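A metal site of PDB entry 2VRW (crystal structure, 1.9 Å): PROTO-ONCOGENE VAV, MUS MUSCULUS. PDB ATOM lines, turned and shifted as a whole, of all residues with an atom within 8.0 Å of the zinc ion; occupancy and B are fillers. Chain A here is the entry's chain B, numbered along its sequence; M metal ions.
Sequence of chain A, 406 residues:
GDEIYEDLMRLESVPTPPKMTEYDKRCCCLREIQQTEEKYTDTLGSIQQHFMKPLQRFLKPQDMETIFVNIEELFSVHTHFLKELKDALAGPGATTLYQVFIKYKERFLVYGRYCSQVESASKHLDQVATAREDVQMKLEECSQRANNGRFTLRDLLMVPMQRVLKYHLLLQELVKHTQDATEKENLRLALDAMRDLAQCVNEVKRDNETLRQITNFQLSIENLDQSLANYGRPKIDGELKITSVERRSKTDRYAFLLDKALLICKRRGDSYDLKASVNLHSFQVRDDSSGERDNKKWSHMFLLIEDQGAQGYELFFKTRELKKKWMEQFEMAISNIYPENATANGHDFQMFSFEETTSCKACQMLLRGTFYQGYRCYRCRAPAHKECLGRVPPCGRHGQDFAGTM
The zinc ion is bound by ND1 of His 385 (2.2 Å), SG of Cys 388 (2.3 Å), SG of Cys 363 (2.3 Å) and SG of Cys 360 (2.3 Å). The zinc ion has four donor atoms within binding distance.
Four residues have an atom within 4 Å of the zinc ion: Cys 360, Cys 363, His 385 and Cys 388.
SG of Cys 360 lies close to N of Ala 362 (3.5 Å). The backbone NH (N) of Met 365 lies close to the side-chain sulfur (SG) of Cys 363, at 3.6 Å. The backbone NH (N) of Cys 360 lies within hydrogen-bond range of the backbone carbonyl oxygen (O) of Met 365. O of Leu 366 lies within hydrogen-bond range of NE2 of His 385, at 2.8 Å.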
ATOM      1  N   SER A 359     -20.090   6.210 -18.673  1.00  0.00           N
ATOM      2  CA  SER A 359     -20.401   6.445 -20.095  1.00  0.00           C
ATOM      3  C   SER A 359     -19.174   6.230 -20.976  1.00  0.00           C
ATOM      4  O   SER A 359     -18.036   6.477 -20.553  1.00  0.00           O
ATOM      5  CB  SER A 359     -20.931   7.868 -20.292  1.00  0.00           C
ATOM      6  OG  SER A 359     -22.235   7.980 -19.769  1.00  0.00           O
ATOM      7  N   CYS A 360     -19.411   5.759 -22.199  1.00  0.00           N
ATOM      8  CA  CYS A 360     -18.350   5.522 -23.175  1.00  0.00           C
ATOM      9  C   CYS A 360     -17.827   6.858 -23.717  1.00  0.00           C
ATOM     10  O   CYS A 360     -18.606   7.740 -24.057  1.00  0.00           O
ATOM     11  CB  CYS A 360     -18.883   4.657 -24.323  1.00  0.00           C
ATOM     12  SG  CYS A 360     -17.760   4.418 -25.750  1.00  0.00           S
ATOM     13  N   LYS A 361     -16.506   6.989 -23.774  1.00  0.00           N
ATOM     14  CA  LYS A 361     -15.869   8.233 -24.200  1.00  0.00           C
ATOM     15  C   LYS A 361     -16.086   8.518 -25.704  1.00  0.00           C
ATOM     16  O   LYS A 361     -16.059   9.678 -26.120  1.00  0.00           O
ATOM     17  CB  LYS A 361     -14.367   8.212 -23.850  1.00  0.00           C
ATOM     18  CG  LYS A 361     -13.613   9.515 -24.094  1.00  0.00           C
ATOM     19  CD  LYS A 361     -13.897  10.570 -23.031  1.00  0.00           C
ATOM     20  CE  LYS A 361     -12.799  11.628 -23.016  1.00  0.00           C
ATOM     21  NZ  LYS A 361     -12.564  12.264 -24.363  1.00  0.00           N
ATOM     22  N   ALA A 362     -16.334   7.481 -26.490  1.00  0.00           N
ATOM     23  CA  ALA A 362     -16.615   7.660 -27.920  1.00  0.00           C
ATOM     24  C   ALA A 362     -18.066   8.021 -28.220  1.00  0.00           C
ATOM     25  O   ALA A 362     -18.333   9.040 -28.863  1.00  0.00           O
ATOM     26  CB  ALA A 362     -16.212   6.426 -28.698  1.00  0.00           C
ATOM     27  N   CYS A 363     -19.009   7.185 -27.770  1.00  0.00           N
ATOM     28  CA  CYS A 363     -20.410   7.307 -28.187  1.00  0.00           C
ATOM     29  C   CYS A 363     -21.331   7.953 -27.134  1.00  0.00           C
ATOM     30  O   CYS A 363     -22.489   8.255 -27.438  1.00  0.00           O
ATOM     31  CB  CYS A 363     -20.962   5.950 -28.621  1.00  0.00           C
ATOM     32  SG  CYS A 363     -21.238   4.784 -27.251  1.00  0.00           S
ATOM     33  N   GLN A 364     -20.804   8.130 -25.921  1.00  0.00           N
ATOM     34  CA  GLN A 364     -21.535   8.772 -24.803  1.00  0.00           C
ATOM     35  C   GLN A 364     -22.673   7.940 -24.203  1.00  0.00           C
ATOM     36  O   GLN A 364     -23.345   8.391 -23.278  1.00  0.00           O
ATOM     37  CB  GLN A 364     -22.003  10.194 -25.159  1.00  0.00           C
ATOM     38  CG  GLN A 364     -20.886  11.147 -25.617  1.00  0.00           C
ATOM     39  CD  GLN A 364     -19.745  11.297 -24.613  1.00  0.00           C
ATOM     40  OE1 GLN A 364     -19.955  11.253 -23.406  1.00  0.00           O
ATOM     41  NE2 GLN A 364     -18.525  11.479 -25.132  1.00  0.00           N
ATOM     42  N   MET A 365     -22.869   6.722 -24.714  1.00  0.00           N
ATOM     43  CA  MET A 365     -23.849   5.790 -24.152  1.00  0.00           C
ATOM     44  C   MET A 365     -23.242   5.002 -22.984  1.00  0.00           C
ATOM     45  O   MET A 365     -22.010   4.912 -22.831  1.00  0.00           O
ATOM     46  CB  MET A 365     -24.368   4.814 -25.222  1.00  0.00           C
ATOM     47  CG  MET A 365     -25.024   5.472 -26.431  1.00  0.00           C
ATOM     48  SD  MET A 365     -26.545   6.330 -26.006  1.00  0.00           S
ATOM     49  CE  MET A 365     -25.999   8.024 -25.964  1.00  0.00           C
ATOM     50  N   LEU A 366     -24.111   4.408 -22.157  1.00  0.00           N
ATOM     51  CA  LEU A 366     -23.661   3.750 -20.942  1.00  0.00           C
ATOM     52  C   LEU A 366     -22.916   2.461 -21.211  1.00  0.00           C
ATOM     53  O   LEU A 366     -23.259   1.723 -22.134  1.00  0.00           O
ATOM     54  CB  LEU A 366     -24.857   3.457 -20.022  1.00  0.00           C
ATOM     55  CG  LEU A 366     -25.521   4.689 -19.386  1.00  0.00           C
ATOM     56  CD1 LEU A 366     -26.785   4.278 -18.665  1.00  0.00           C
ATOM     57  CD2 LEU A 366     -24.557   5.377 -18.447  1.00  0.00           C
ATOM     58  N   LEU A 367     -21.873   2.204 -20.434  1.00  0.00           N
ATOM     59  CA  LEU A 367     -21.312   0.864 -20.352  1.00  0.00           C
ATOM     60  C   LEU A 367     -22.371  -0.017 -19.674  1.00  0.00           C
ATOM     61  O   LEU A 367     -22.992   0.394 -18.681  1.00  0.00           O
ATOM     62  CB  LEU A 367     -19.994   0.876 -19.563  1.00  0.00           C
ATOM     63  CG  LEU A 367     -18.775   1.281 -20.394  1.00  0.00           C
ATOM     64  CD1 LEU A 367     -18.936   2.635 -21.043  1.00  0.00           C
ATOM     65  CD2 LEU A 367     -17.574   1.305 -19.525  1.00  0.00           C
ATOM     66  N   ARG A 368     -22.574  -1.215 -20.232  1.00  0.00           N
ATOM     67  CA  ARG A 368     -23.759  -2.013 -19.928  1.00  0.00           C
ATOM     68  C   ARG A 368     -23.419  -3.308 -19.210  1.00  0.00           C
ATOM     69  O   ARG A 368     -22.488  -4.011 -19.591  1.00  0.00           O
ATOM     70  CB  ARG A 368     -24.534  -2.333 -21.217  1.00  0.00           C
ATOM     71  CG  ARG A 368     -24.710  -1.107 -22.087  1.00  0.00           C
ATOM     72  CD  ARG A 368     -25.767  -1.257 -23.144  1.00  0.00           C
ATOM     73  NE  ARG A 368     -25.773  -0.077 -24.013  1.00  0.00           N
ATOM     74  CZ  ARG A 368     -25.047   0.038 -25.133  1.00  0.00           C
ATOM     75  NH1 ARG A 368     -24.278  -0.960 -25.552  1.00  0.00           N
ATOM     76  NH2 ARG A 368     -25.115   1.167 -25.830  1.00  0.00           N
ATOM     77  N   PRO A 383     -13.086   5.310 -20.462  1.00  0.00           N
ATOM     78  CA  PRO A 383     -13.903   4.108 -20.620  1.00  0.00           C
ATOM     79  C   PRO A 383     -14.467   4.000 -22.031  1.00  0.00           C
ATOM     80  O   PRO A 383     -14.735   5.034 -22.657  1.00  0.00           O
ATOM     81  CB  PRO A 383     -15.053   4.302 -19.627  1.00  0.00           C
ATOM     82  CG  PRO A 383     -14.971   5.739 -19.164  1.00  0.00           C
ATOM     83  CD  PRO A 383     -13.846   6.424 -19.870  1.00  0.00           C
ATOM     84  N   ALA A 384     -14.659   2.779 -22.533  1.00  0.00           N
ATOM     85  CA  ALA A 384     -15.184   2.574 -23.881  1.00  0.00           C
ATOM     86  C   ALA A 384     -15.784   1.179 -24.064  1.00  0.00           C
ATOM     87  O   ALA A 384     -15.322   0.208 -23.440  1.00  0.00           O
ATOM     88  CB  ALA A 384     -14.096   2.817 -24.927  1.00  0.00           C
ATOM     89  N   HIS A 385     -16.801   1.099 -24.930  1.00  0.00           N
ATOM     90  CA  HIS A 385     -17.359  -0.174 -25.353  1.00  0.00           C
ATOM     91  C   HIS A 385     -16.331  -0.864 -26.247  1.00  0.00           C
ATOM     92  O   HIS A 385     -15.557  -0.190 -26.931  1.00  0.00           O
ATOM     93  CB  HIS A 385     -18.625   0.031 -26.193  1.00  0.00           C
ATOM     94  CG  HIS A 385     -19.772   0.677 -25.464  1.00  0.00           C
ATOM     95  ND1 HIS A 385     -20.214   1.943 -25.762  1.00  0.00           N
ATOM     96  CD2 HIS A 385     -20.597   0.199 -24.498  1.00  0.00           C
ATOM     97  CE1 HIS A 385     -21.256   2.237 -24.996  1.00  0.00           C
ATOM     98  NE2 HIS A 385     -21.506   1.193 -24.221  1.00  0.00           N
ATOM     99  N   LYS A 386     -16.353  -2.201 -26.280  1.00  0.00           N
ATOM    100  CA  LYS A 386     -15.472  -2.951 -27.199  1.00  0.00           C
ATOM    101  C   LYS A 386     -15.542  -2.432 -28.637  1.00  0.00           C
ATOM    102  O   LYS A 386     -14.514  -2.303 -29.320  1.00  0.00           O
ATOM    103  CB  LYS A 386     -15.774  -4.461 -27.161  1.00  0.00           C
ATOM    104  CG  LYS A 386     -14.727  -5.337 -27.837  1.00  0.00           C
ATOM    105  CD  LYS A 386     -15.058  -6.836 -27.717  1.00  0.00           C
ATOM    106  CE  LYS A 386     -14.010  -7.694 -28.455  1.00  0.00           C
ATOM    107  NZ  LYS A 386     -14.335  -9.160 -28.403  1.00  0.00           N
ATOM    108  N   GLU A 387     -16.754  -2.107 -29.092  1.00  0.00           N
ATOM    109  CA  GLU A 387     -16.994  -1.687 -30.482  1.00  0.00           C
ATOM    110  C   GLU A 387     -16.549  -0.257 -30.782  1.00  0.00           C
ATOM    111  O   GLU A 387     -16.532   0.161 -31.950  1.00  0.00           O
ATOM    112  CB  GLU A 387     -18.485  -1.839 -30.821  1.00  0.00           C
ATOM    113  CG  GLU A 387     -19.064  -3.246 -30.645  1.00  0.00           C
ATOM    114  CD  GLU A 387     -19.678  -3.483 -29.273  1.00  0.00           C
ATOM    115  OE1 GLU A 387     -19.306  -2.864 -28.270  1.00  0.00           O
ATOM    116  OE2 GLU A 387     -20.638  -4.401 -29.219  1.00  0.00           O
ATOM    117  N   CYS A 388     -16.191   0.486 -29.739  1.00  0.00           N
ATOM    118  CA  CYS A 388     -15.964   1.938 -29.816  1.00  0.00           C
ATOM    119  C   CYS A 388     -14.501   2.368 -29.680  1.00  0.00           C
ATOM    120  O   CYS A 388     -14.192   3.554 -29.773  1.00  0.00           O
ATOM    121  CB  CYS A 388     -16.780   2.642 -28.735  1.00  0.00           C
ATOM    122  SG  CYS A 388     -18.554   2.649 -29.060  1.00  0.00           S
ATOM    123  N   LEU A 389     -13.618   1.396 -29.456  1.00  0.00           N
ATOM    124  CA  LEU A 389     -12.216   1.672 -29.118  1.00  0.00           C
ATOM    125  C   LEU A 389     -11.481   2.539 -30.145  1.00  0.00           C
ATOM    126  O   LEU A 389     -10.719   3.433 -29.765  1.00  0.00           O
ATOM    127  CB  LEU A 389     -11.443   0.378 -28.893  1.00  0.00           C
ATOM    128  CG  LEU A 389     -11.967  -0.546 -27.795  1.00  0.00           C
ATOM    129  CD1 LEU A 389     -10.988  -1.694 -27.625  1.00  0.00           C
ATOM    130  CD2 LEU A 389     -12.148   0.178 -26.474  1.00  0.00           C
ATOM    131  N   ARG A 391     -12.780   4.736 -31.962  1.00  0.00           N
ATOM    132  CA  ARG A 391     -13.466   6.018 -32.111  1.00  0.00           C
ATOM    133  C   ARG A 391     -13.301   6.943 -30.908  1.00  0.00           C
ATOM    134  O   ARG A 391     -13.817   8.064 -30.907  1.00  0.00           O
ATOM    135  CB  ARG A 391     -14.946   5.804 -32.454  1.00  0.00           C
ATOM    136  CG  ARG A 391     -15.178   5.313 -33.877  1.00  0.00           C
ATOM    137  CD  ARG A 391     -16.568   5.662 -34.361  1.00  0.00           C
ATOM    138  NE  ARG A 391     -16.734   5.424 -35.806  1.00  0.00           N
ATOM    139  CZ  ARG A 391     -17.433   4.420 -36.327  1.00  0.00           C
ATOM    140  NH1 ARG A 391     -18.044   3.538 -35.542  1.00  0.00           N
ATOM    141  NH2 ARG A 391     -17.525   4.300 -37.642  1.00  0.00           N
ATOM    142  N   VAL A 392     -12.577   6.490 -29.885  1.00  0.00           N
ATOM    143  CA  VAL A 392     -12.226   7.339 -28.755  1.00  0.00           C
ATOM    144  C   VAL A 392     -11.167   8.357 -29.214  1.00  0.00           C
ATOM    145  O   VAL A 392     -10.178   7.972 -29.836  1.00  0.00           O
ATOM    146  CB  VAL A 392     -11.698   6.490 -27.548  1.00  0.00           C
ATOM    147  CG1 VAL A 392     -11.380   7.387 -26.344  1.00  0.00           C
ATOM    148  CG2 VAL A 392     -12.726   5.434 -27.160  1.00  0.00           C
HETATM  149 ZN    ZN M   1     -19.392   3.434 -27.086  1.00  0.00          ZN
